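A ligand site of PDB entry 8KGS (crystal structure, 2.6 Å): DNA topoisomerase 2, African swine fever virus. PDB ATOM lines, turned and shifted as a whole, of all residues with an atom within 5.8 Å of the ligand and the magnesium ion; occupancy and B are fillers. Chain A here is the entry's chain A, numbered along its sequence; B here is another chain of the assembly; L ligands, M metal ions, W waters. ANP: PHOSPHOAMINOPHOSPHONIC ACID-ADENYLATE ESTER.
Glu 60 touches the magnesium ion (OE2 to MG, 3.8 Å). The nearest printed residue that does not touch the magnesium ion is Gly 147 (4.4 Å).
The magnesium ion is bound by the side-chain amide oxygen (OD1) of Asn 64 (2.1 Å), water W4 (2.1 Å), an oxygen (O1G) of the ligand (2.1 Å), water W3 (2.1 Å), an oxygen (O2A) of the ligand (2.1 Å) and an oxygen (O1B) of the ligand (2.2 Å). The magnesium ion has six donor atoms within binding distance.
Water W3 bridges OD2 of Asp 67 (3.1 Å) and N of Gly 142 (3.4 Å). Water W4 lies within hydrogen-bond range of OE2 of Glu 60 and ND2 of Asn 64. Water W1 bridges NZ of Lys 368 (2.5 Å) and OE2 of Glu 60 (3.0 Å).
The side-chain carboxylate (OE2) of Glu 60 sits close to an oxygen (O1G) of the ligand (3.5 Å). ND1 of His 68 touches C2 of the ligand (3.4 Å). Ile 100 touches the ligand. Ala 122 touches the ligand. Ala 128 touches the ligand. Gly 129 touches the ligand (CA to O3', 3.6 Å). Gly 142 touches the ligand (CA to N3B, 3.4 Å). Thr 193 touches the ligand. Gln 366 touches the ligand. CZ of Phe 4 of chain B touches O2' of the ligand (3.4 Å). Hydrophobic or aromatic side chains that line the ligand: His 68, Ile 100, Ala 122, Val 146, Leu 148 and Phe 4 of chain B. Of the 31 residues printed, 22 come within 4 Å of the ligand. Along chain A the residues within 4 Å of the ligand span positions 60 to 368.
An oxygen (O3G) of the ligand is in hydrogen-bond range of the backbone NH of Val 146 (2.5 Å). An oxygen (O1A) of the ligand is in salt-bridge range of the side-chain amino group (NZ) of Lys 149, at 2.6 Å. The side-chain amide nitrogen (ND2) of Asn 131 sits at hydrogen-bond distance from an oxygen (O2B) of the ligand, 2.7 Å away. A nitrogen (N6) of the ligand is in hydrogen-bond range of the side-chain amide oxygen of Asn 95 (2.7 Å). The backbone NH of Gly 147 sits at hydrogen-bond distance from an oxygen (O3G) of the ligand (2.8 Å). An oxygen (O3') of the ligand lies within hydrogen-bond range of the backbone NH (N) of Thr 130 (3.0 Å). The side-chain hydroxyl of Thr 130 sits at hydrogen-bond distance from an oxygen (O2') of the ligand, 2.8 Å away. NZ of Lys 368 is in salt-bridge range of O2G of the ligand (2.8 Å). The backbone NH (N) of Thr 143 lies within hydrogen-bond range of an oxygen (O2G) of the ligand, 2.9 Å away. N of Gly 145 is in hydrogen-bond range of O3G of the ligand, at 3.1 Å. An oxygen (O2G) of the ligand sits at hydrogen-bond distance from the backbone NH (N) of Asn 144, 3.0 Å away. The backbone NH (N) of Leu 148 is in hydrogen-bond range of an oxygen (O1A) of the ligand (3.1 Å).
The side-chain amino group (NZ) of Lys 149 sits at hydrogen-bond distance from the backbone carbonyl oxygen (O) of Gly 145, at 2.6 Å. The backbone carbonyl oxygen (O) of Ala 122 sits close to the side-chain amino group (NZ) of Lys 149. The backbone NH (N) of Asn 95 sits at hydrogen-bond distance from the backbone carbonyl oxygen (O) of Thr 193. N of Ala 128 lies within hydrogen-bond range of O of Gly 145, 3.0 Å away. ND2 of Asn 144 lies within hydrogen-bond range of OE1 of Gln 366, 2.7 Å away. The side-chain carboxylate (OD2) of Asp 67 is in hydrogen-bond range of the backbone NH (N) of Gly 142 (2.8 Å). A ring nitrogen (NE2) of His 68 sits at hydrogen-bond distance from the backbone carbonyl oxygen (O) of Pro 98 (2.6 Å). The side-chain carboxylate (OE1) of Glu 60 is in hydrogen-bond range of the side-chain amide nitrogen (NE2) of Gln 366 (2.7 Å).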
ATOM      1  N   GLU A  60      -0.369  32.773  32.418  1.00  0.00           N
ATOM      2  CA  GLU A  60      -1.161  31.683  31.837  1.00  0.00           C
ATOM      3  C   GLU A  60      -0.317  30.433  31.642  1.00  0.00           C
ATOM      4  O   GLU A  60      -0.721  29.331  32.026  1.00  0.00           O
ATOM      5  CB  GLU A  60      -1.790  32.135  30.530  1.00  0.00           C
ATOM      6  CG  GLU A  60      -2.874  33.214  30.683  1.00  0.00           C
ATOM      7  CD  GLU A  60      -4.155  32.708  31.332  1.00  0.00           C
ATOM      8  OE1 GLU A  60      -5.033  33.547  31.662  1.00  0.00           O
ATOM      9  OE2 GLU A  60      -4.294  31.480  31.536  1.00  0.00           O
ATOM     10  N   ILE A  61       0.889  30.595  31.147  1.00  0.00           N
ATOM     11  CA  ILE A  61       1.762  29.489  30.956  1.00  0.00           C
ATOM     12  C   ILE A  61       2.299  28.937  32.273  1.00  0.00           C
ATOM     13  O   ILE A  61       2.454  27.752  32.423  1.00  0.00           O
ATOM     14  CB  ILE A  61       2.915  29.919  30.019  1.00  0.00           C
ATOM     15  CG1 ILE A  61       2.403  30.257  28.631  1.00  0.00           C
ATOM     16  CG2 ILE A  61       3.961  28.818  29.906  1.00  0.00           C
ATOM     17  CD1 ILE A  61       3.318  31.184  27.885  1.00  0.00           C
ATOM     18  N   VAL A  63       0.721  28.946  35.158  1.00  0.00           N
ATOM     19  CA  VAL A  63      -0.347  28.192  35.806  1.00  0.00           C
ATOM     20  C   VAL A  63      -0.670  26.919  35.022  1.00  0.00           C
ATOM     21  O   VAL A  63      -1.076  25.915  35.608  1.00  0.00           O
ATOM     22  CB  VAL A  63      -1.597  29.070  36.053  1.00  0.00           C
ATOM     23  CG1 VAL A  63      -2.765  28.235  36.634  1.00  0.00           C
ATOM     24  CG2 VAL A  63      -1.259  30.236  36.985  1.00  0.00           C
ATOM     25  N   ASN A  64      -0.463  26.922  33.702  1.00  0.00           N
ATOM     26  CA  ASN A  64      -0.574  25.653  32.977  1.00  0.00           C
ATOM     27  C   ASN A  64       0.441  24.636  33.492  1.00  0.00           C
ATOM     28  O   ASN A  64       0.105  23.460  33.686  1.00  0.00           O
ATOM     29  CB  ASN A  64      -0.402  25.892  31.474  1.00  0.00           C
ATOM     30  CG  ASN A  64      -1.656  26.431  30.837  1.00  0.00           C
ATOM     31  OD1 ASN A  64      -2.762  26.287  31.383  1.00  0.00           O
ATOM     32  ND2 ASN A  64      -1.505  27.039  29.679  1.00  0.00           N
ATOM     33  N   ALA A  65       1.660  25.087  33.756  1.00  0.00           N
ATOM     34  CA  ALA A  65       2.698  24.185  34.257  1.00  0.00           C
ATOM     35  C   ALA A  65       2.365  23.661  35.657  1.00  0.00           C
ATOM     36  O   ALA A  65       2.515  22.463  35.938  1.00  0.00           O
ATOM     37  CB  ALA A  65       4.039  24.912  34.255  1.00  0.00           C
ATOM     38  N   ASP A  67      -0.556  23.458  36.920  1.00  0.00           N
ATOM     39  CA  ASP A  67      -1.703  22.573  36.691  1.00  0.00           C
ATOM     40  C   ASP A  67      -1.236  21.173  36.323  1.00  0.00           C
ATOM     41  O   ASP A  67      -1.749  20.183  36.855  1.00  0.00           O
ATOM     42  CB  ASP A  67      -2.574  23.162  35.589  1.00  0.00           C
ATOM     43  CG  ASP A  67      -3.457  24.271  36.083  1.00  0.00           C
ATOM     44  OD1 ASP A  67      -3.501  24.518  37.321  1.00  0.00           O
ATOM     45  OD2 ASP A  67      -4.125  24.917  35.241  1.00  0.00           O
ATOM     46  N   HIS A  68      -0.292  21.079  35.382  1.00  0.00           N
ATOM     47  CA  HIS A  68       0.248  19.774  35.011  1.00  0.00           C
ATOM     48  C   HIS A  68       0.880  19.102  36.232  1.00  0.00           C
ATOM     49  O   HIS A  68       0.732  17.893  36.428  1.00  0.00           O
ATOM     50  CB  HIS A  68       1.267  19.898  33.885  1.00  0.00           C
ATOM     51  CG  HIS A  68       1.452  18.632  33.092  1.00  0.00           C
ATOM     52  ND1 HIS A  68       0.388  17.842  32.701  1.00  0.00           N
ATOM     53  CD2 HIS A  68       2.566  18.017  32.635  1.00  0.00           C
ATOM     54  CE1 HIS A  68       0.840  16.803  32.019  1.00  0.00           C
ATOM     55  NE2 HIS A  68       2.165  16.878  31.981  1.00  0.00           N
ATOM     56  N   ASN A  95       8.237  22.134  31.536  1.00  0.00           N
ATOM     57  CA  ASN A  95       7.961  21.141  32.574  1.00  0.00           C
ATOM     58  C   ASN A  95       8.234  19.741  32.041  1.00  0.00           C
ATOM     59  O   ASN A  95       8.305  19.526  30.827  1.00  0.00           O
ATOM     60  CB  ASN A  95       6.504  21.259  33.062  1.00  0.00           C
ATOM     61  CG  ASN A  95       5.508  21.012  31.964  1.00  0.00           C
ATOM     62  OD1 ASN A  95       4.937  21.959  31.410  1.00  0.00           O
ATOM     63  ND2 ASN A  95       5.285  19.731  31.636  1.00  0.00           N
ATOM     64  N   PRO A  98       4.416  13.949  31.653  1.00  0.00           N
ATOM     65  CA  PRO A  98       4.046  13.516  30.300  1.00  0.00           C
ATOM     66  C   PRO A  98       3.771  14.726  29.431  1.00  0.00           C
ATOM     67  O   PRO A  98       3.226  15.725  29.903  1.00  0.00           O
ATOM     68  CB  PRO A  98       2.789  12.669  30.523  1.00  0.00           C
ATOM     69  CG  PRO A  98       2.868  12.236  31.959  1.00  0.00           C
ATOM     70  CD  PRO A  98       3.504  13.402  32.679  1.00  0.00           C
ATOM     71  N   GLY A  99       4.202  14.669  28.176  1.00  0.00           N
ATOM     72  CA  GLY A  99       3.975  15.756  27.244  1.00  0.00           C
ATOM     73  C   GLY A  99       2.525  15.840  26.793  1.00  0.00           C
ATOM     74  O   GLY A  99       1.676  15.030  27.146  1.00  0.00           O
ATOM     75  N   ILE A 100       2.251  16.842  25.977  1.00  0.00           N
ATOM     76  CA  ILE A 100       0.915  16.927  25.381  1.00  0.00           C
ATOM     77  C   ILE A 100       0.773  15.831  24.321  1.00  0.00           C
ATOM     78  O   ILE A 100       1.712  15.638  23.518  1.00  0.00           O
ATOM     79  CB  ILE A 100       0.677  18.310  24.782  1.00  0.00           C
ATOM     80  CG1 ILE A 100       0.851  19.378  25.882  1.00  0.00           C
ATOM     81  CG2 ILE A 100      -0.695  18.390  24.149  1.00  0.00           C
ATOM     82  CD1 ILE A 100       0.373  20.750  25.479  1.00  0.00           C
ATOM     83  N   ALA A 122      -4.590  22.784  21.568  1.00  0.00           N
ATOM     84  CA  ALA A 122      -4.252  23.321  22.877  1.00  0.00           C
ATOM     85  C   ALA A 122      -3.677  24.722  22.812  1.00  0.00           C
ATOM     86  O   ALA A 122      -3.824  25.486  23.769  1.00  0.00           O
ATOM     87  CB  ALA A 122      -3.262  22.387  23.582  1.00  0.00           C
ATOM     88  N   SER A 123      -3.010  25.093  21.714  1.00  0.00           N
ATOM     89  CA  SER A 123      -2.355  26.395  21.659  1.00  0.00           C
ATOM     90  C   SER A 123      -3.014  27.419  20.748  1.00  0.00           C
ATOM     91  O   SER A 123      -2.751  28.615  20.907  1.00  0.00           O
ATOM     92  CB  SER A 123      -0.875  26.246  21.226  1.00  0.00           C
ATOM     93  OG  SER A 123      -0.740  25.396  20.111  1.00  0.00           O
ATOM     94  N   ALA A 128     -10.759  25.578  24.269  1.00  0.00           N
ATOM     95  CA  ALA A 128     -10.339  24.215  23.971  1.00  0.00           C
ATOM     96  C   ALA A 128      -9.278  23.788  24.972  1.00  0.00           C
ATOM     97  O   ALA A 128      -8.359  24.557  25.277  1.00  0.00           O
ATOM     98  CB  ALA A 128      -9.805  24.110  22.540  1.00  0.00           C
ATOM     99  N   GLY A 129      -9.407  22.570  25.473  1.00  0.00           N
ATOM    100  CA  GLY A 129      -8.481  22.056  26.462  1.00  0.00           C
ATOM    101  C   GLY A 129      -9.071  20.844  27.169  1.00  0.00           C
ATOM    102  O   GLY A 129     -10.072  20.267  26.744  1.00  0.00           O
ATOM    103  N   THR A 130      -8.412  20.449  28.253  1.00  0.00           N
ATOM    104  CA  THR A 130      -8.846  19.290  29.019  1.00  0.00           C
ATOM    105  C   THR A 130      -9.734  19.663  30.199  1.00  0.00           C
ATOM    106  O   THR A 130     -10.076  18.784  31.005  1.00  0.00           O
ATOM    107  CB  THR A 130      -7.647  18.461  29.511  1.00  0.00           C
ATOM    108  OG1 THR A 130      -6.747  19.292  30.239  1.00  0.00           O
ATOM    109  CG2 THR A 130      -6.911  17.837  28.343  1.00  0.00           C
ATOM    110  N   ASN A 131     -10.114  20.936  30.341  1.00  0.00           N
ATOM    111  CA  ASN A 131     -10.875  21.370  31.503  1.00  0.00           C
ATOM    112  C   ASN A 131     -12.231  21.956  31.133  1.00  0.00           C
ATOM    113  O   ASN A 131     -12.901  22.529  31.998  1.00  0.00           O
ATOM    114  CB  ASN A 131     -10.084  22.376  32.325  1.00  0.00           C
ATOM    115  CG  ASN A 131      -8.763  21.817  32.790  1.00  0.00           C
ATOM    116  OD1 ASN A 131      -8.722  20.809  33.540  1.00  0.00           O
ATOM    117  ND2 ASN A 131      -7.658  22.433  32.324  1.00  0.00           N
ATOM    118  N   GLY A 141      -5.965  25.373  38.256  1.00  0.00           N
ATOM    119  CA  GLY A 141      -6.431  26.697  37.919  1.00  0.00           C
ATOM    120  C   GLY A 141      -7.149  26.719  36.585  1.00  0.00           C
ATOM    121  O   GLY A 141      -8.149  27.424  36.417  1.00  0.00           O
ATOM    122  N   GLY A 142      -6.660  25.934  35.629  1.00  0.00           N
ATOM    123  CA  GLY A 142      -7.212  25.994  34.280  1.00  0.00           C
ATOM    124  C   GLY A 142      -8.679  25.585  34.256  1.00  0.00           C
ATOM    125  O   GLY A 142      -9.093  24.649  34.957  1.00  0.00           O
ATOM    126  N   THR A 143      -9.456  26.290  33.451  1.00  0.00           N
ATOM    127  CA  THR A 143     -10.851  25.914  33.320  1.00  0.00           C
ATOM    128  C   THR A 143     -11.407  26.294  31.943  1.00  0.00           C
ATOM    129  O   THR A 143     -12.275  25.593  31.417  1.00  0.00           O
ATOM    130  CB  THR A 143     -11.682  26.542  34.459  1.00  0.00           C
ATOM    131  OG1 THR A 143     -13.054  26.172  34.343  1.00  0.00           O
ATOM    132  CG2 THR A 143     -11.569  28.060  34.482  1.00  0.00           C
ATOM    133  N   ASN A 144     -10.885  27.364  31.326  1.00  0.00           N
ATOM    134  CA  ASN A 144     -11.551  28.000  30.186  1.00  0.00           C
ATOM    135  C   ASN A 144     -11.078  27.514  28.811  1.00  0.00           C
ATOM    136  O   ASN A 144     -11.785  27.748  27.824  1.00  0.00           O
ATOM    137  CB  ASN A 144     -11.372  29.514  30.254  1.00  0.00           C
ATOM    138  CG  ASN A 144     -12.100  30.110  31.433  1.00  0.00           C
ATOM    139  OD1 ASN A 144     -13.240  29.743  31.698  1.00  0.00           O
ATOM    140  ND2 ASN A 144     -11.447  31.017  32.149  1.00  0.00           N
ATOM    141  N   GLY A 145      -9.932  26.855  28.728  1.00  0.00           N
ATOM    142  CA  GLY A 145      -9.378  26.548  27.411  1.00  0.00           C
ATOM    143  C   GLY A 145      -8.996  27.795  26.636  1.00  0.00           C
ATOM    144  O   GLY A 145      -9.180  27.834  25.406  1.00  0.00           O
ATOM    145  N   VAL A 146      -8.455  28.807  27.323  1.00  0.00           N
ATOM    146  CA  VAL A 146      -8.233  30.097  26.682  1.00  0.00           C
ATOM    147  C   VAL A 146      -6.807  30.603  26.925  1.00  0.00           C
ATOM    148  O   VAL A 146      -6.214  31.221  26.027  1.00  0.00           O
ATOM    149  CB  VAL A 146      -9.292  31.129  27.156  1.00  0.00           C
ATOM    150  CG1 VAL A 146      -8.865  32.546  26.875  1.00  0.00           C
ATOM    151  CG2 VAL A 146     -10.631  30.863  26.479  1.00  0.00           C
ATOM    152  N   GLY A 147      -6.250  30.342  28.111  1.00  0.00           N
ATOM    153  CA  GLY A 147      -5.023  31.030  28.519  1.00  0.00           C
ATOM    154  C   GLY A 147      -3.878  30.898  27.525  1.00  0.00           C
ATOM    155  O   GLY A 147      -3.219  31.895  27.164  1.00  0.00           O
ATOM    156  N   LEU A 148      -3.625  29.666  27.061  1.00  0.00           N
ATOM    157  CA  LEU A 148      -2.488  29.439  26.169  1.00  0.00           C
ATOM    158  C   LEU A 148      -2.636  30.235  24.877  1.00  0.00           C
ATOM    159  O   LEU A 148      -1.662  30.819  24.372  1.00  0.00           O
ATOM    160  CB  LEU A 148      -2.338  27.934  25.888  1.00  0.00           C
ATOM    161  CG  LEU A 148      -1.116  27.511  25.061  1.00  0.00           C
ATOM    162  CD1 LEU A 148       0.093  28.369  25.403  1.00  0.00           C
ATOM    163  CD2 LEU A 148      -0.796  26.004  25.232  1.00  0.00           C
ATOM    164  N   LYS A 149      -3.862  30.314  24.352  1.00  0.00           N
ATOM    165  CA  LYS A 149      -4.051  31.056  23.105  1.00  0.00           C
ATOM    166  C   LYS A 149      -3.921  32.553  23.359  1.00  0.00           C
ATOM    167  O   LYS A 149      -3.560  33.290  22.448  1.00  0.00           O
ATOM    168  CB  LYS A 149      -5.413  30.734  22.470  1.00  0.00           C
ATOM    169  CG  LYS A 149      -5.631  29.258  22.222  1.00  0.00           C
ATOM    170  CD  LYS A 149      -6.207  28.654  23.470  1.00  0.00           C
ATOM    171  CE  LYS A 149      -6.257  27.182  23.413  1.00  0.00           C
ATOM    172  NZ  LYS A 149      -6.943  26.758  24.652  1.00  0.00           N
ATOM    173  N   THR A 193       7.245  19.526  28.120  1.00  0.00           N
ATOM    174  CA  THR A 193       6.530  20.565  27.392  1.00  0.00           C
ATOM    175  C   THR A 193       7.242  21.897  27.593  1.00  0.00           C
ATOM    176  O   THR A 193       7.595  22.248  28.729  1.00  0.00           O
ATOM    177  CB  THR A 193       5.087  20.658  27.856  1.00  0.00           C
ATOM    178  OG1 THR A 193       4.496  19.346  27.781  1.00  0.00           O
ATOM    179  CG2 THR A 193       4.318  21.647  26.994  1.00  0.00           C
ATOM    180  N   ILE A 195       7.033  26.056  26.246  1.00  0.00           N
ATOM    181  CA  ILE A 195       6.532  27.203  25.494  1.00  0.00           C
ATOM    182  C   ILE A 195       7.616  28.283  25.520  1.00  0.00           C
ATOM    183  O   ILE A 195       8.126  28.641  26.601  1.00  0.00           O
ATOM    184  CB  ILE A 195       5.212  27.754  26.066  1.00  0.00           C
ATOM    185  CG1 ILE A 195       4.192  26.637  26.338  1.00  0.00           C
ATOM    186  CG2 ILE A 195       4.664  28.859  25.152  1.00  0.00           C
ATOM    187  CD1 ILE A 195       3.855  25.761  25.133  1.00  0.00           C
ATOM    188  N   GLN A 366     -11.571  35.635  33.297  1.00  0.00           N
ATOM    189  CA  GLN A 366     -10.413  34.847  32.879  1.00  0.00           C
ATOM    190  C   GLN A 366      -9.177  35.174  33.715  1.00  0.00           C
ATOM    191  O   GLN A 366      -8.395  34.279  34.036  1.00  0.00           O
ATOM    192  CB  GLN A 366     -10.131  35.063  31.388  1.00  0.00           C
ATOM    193  CG  GLN A 366      -8.757  34.577  30.933  1.00  0.00           C
ATOM    194  CD  GLN A 366      -8.645  33.066  30.909  1.00  0.00           C
ATOM    195  OE1 GLN A 366      -9.614  32.357  30.630  1.00  0.00           O
ATOM    196  NE2 GLN A 366      -7.462  32.557  31.208  1.00  0.00           N
ATOM    197  N   LYS A 368      -8.792  35.686  36.677  1.00  0.00           N
ATOM    198  CA  LYS A 368      -8.821  35.016  37.976  1.00  0.00           C
ATOM    199  C   LYS A 368      -8.204  35.902  39.057  1.00  0.00           C
ATOM    200  O   LYS A 368      -7.345  35.462  39.844  1.00  0.00           O
ATOM    201  CB  LYS A 368      -8.140  33.650  37.889  1.00  0.00           C
ATOM    202  CG  LYS A 368      -8.803  32.778  36.833  1.00  0.00           C
ATOM    203  CD  LYS A 368      -8.050  31.463  36.629  1.00  0.00           C
ATOM    204  CE  LYS A 368      -8.611  30.728  35.433  1.00  0.00           C
ATOM    205  NZ  LYS A 368      -7.532  30.446  34.465  1.00  0.00           N
ATOM    206  N   PHE B   4      -9.297  16.133  25.211  1.00  0.00           N
ATOM    207  CA  PHE B   4      -9.226  17.512  24.803  1.00  0.00           C
ATOM    208  C   PHE B   4     -10.472  17.884  24.076  1.00  0.00           C
ATOM    209  O   PHE B   4     -10.778  17.323  23.041  1.00  0.00           O
ATOM    210  CB  PHE B   4      -8.021  17.700  23.881  1.00  0.00           C
ATOM    211  CG  PHE B   4      -6.731  17.954  24.573  1.00  0.00           C
ATOM    212  CD1 PHE B   4      -6.185  19.224  24.576  1.00  0.00           C
ATOM    213  CD2 PHE B   4      -6.031  16.932  25.172  1.00  0.00           C
ATOM    214  CE1 PHE B   4      -4.978  19.467  25.187  1.00  0.00           C
ATOM    215  CE2 PHE B   4      -4.823  17.170  25.797  1.00  0.00           C
ATOM    216  CZ  PHE B   4      -4.296  18.442  25.802  1.00  0.00           C
HETATM  217  PG  ANP L   1      -7.610  28.311  31.136  1.00  0.00           P
HETATM  218  O1G ANP L   1      -6.148  28.552  31.364  1.00  0.00           O
HETATM  219  O2G ANP L   1      -8.434  28.802  32.383  1.00  0.00           O
HETATM  220  O3G ANP L   1      -8.020  29.065  29.813  1.00  0.00           O
HETATM  221  PB  ANP L   1      -6.771  25.723  30.318  1.00  0.00           P
HETATM  222  O1B ANP L   1      -5.447  25.883  31.048  1.00  0.00           O
HETATM  223  O2B ANP L   1      -7.317  24.277  30.410  1.00  0.00           O
HETATM  224  N3B ANP L   1      -7.967  26.663  30.996  1.00  0.00           N
HETATM  225  PA  ANP L   1      -5.220  26.501  28.109  1.00  0.00           P
HETATM  226  O1A ANP L   1      -5.564  27.236  26.849  1.00  0.00           O
HETATM  227  O2A ANP L   1      -4.397  27.334  29.108  1.00  0.00           O
HETATM  228  O3A ANP L   1      -6.608  26.067  28.800  1.00  0.00           O
HETATM  229  O5' ANP L   1      -4.457  25.159  27.691  1.00  0.00           O
HETATM  230  C5' ANP L   1      -5.084  24.218  26.818  1.00  0.00           C
HETATM  231  C4' ANP L   1      -4.740  22.827  27.300  1.00  0.00           C
HETATM  232  O4' ANP L   1      -3.361  22.555  26.989  1.00  0.00           O
HETATM  233  C3' ANP L   1      -4.841  22.592  28.799  1.00  0.00           C
HETATM  234  O3' ANP L   1      -6.181  22.277  29.190  1.00  0.00           O
HETATM  235  C2' ANP L   1      -3.907  21.399  29.009  1.00  0.00           C
HETATM  236  O2' ANP L   1      -4.595  20.172  28.732  1.00  0.00           O
HETATM  237  C1' ANP L   1      -2.830  21.618  27.928  1.00  0.00           C
HETATM  238  N9  ANP L   1      -1.579  22.154  28.437  1.00  0.00           N
HETATM  239  C8  ANP L   1      -1.172  23.459  28.427  1.00  0.00           C
HETATM  240  N7  ANP L   1       0.008  23.661  28.951  1.00  0.00           N
HETATM  241  C5  ANP L   1       0.408  22.394  29.352  1.00  0.00           C
HETATM  242  C6  ANP L   1       1.578  21.925  29.982  1.00  0.00           C
HETATM  243  N6  ANP L   1       2.588  22.708  30.353  1.00  0.00           N
HETATM  244  N1  ANP L   1       1.657  20.596  30.238  1.00  0.00           N
HETATM  245  C2  ANP L   1       0.638  19.800  29.886  1.00  0.00           C
HETATM  246  N3  ANP L   1      -0.506  20.135  29.281  1.00  0.00           N
HETATM  247  C4  ANP L   1      -0.562  21.461  29.045  1.00  0.00           C
HETATM  248 MG    MG M   1      -4.266  27.679  31.210  1.00  0.00          MG
HETATM  249  O   HOH W   1      -5.046  30.161  34.087  1.00  0.00           O
HETATM  250  O   HOH W   2      -9.907  23.458  29.164  1.00  0.00           O
HETATM  251  O   HOH W   3      -4.641  27.227  33.234  1.00  0.00           O
HETATM  252  O   HOH W   4      -2.975  29.262  31.474  1.00  0.00           O
HETATM  253  O   HOH W   5      -3.985  23.719  32.448  1.00  0.00           O
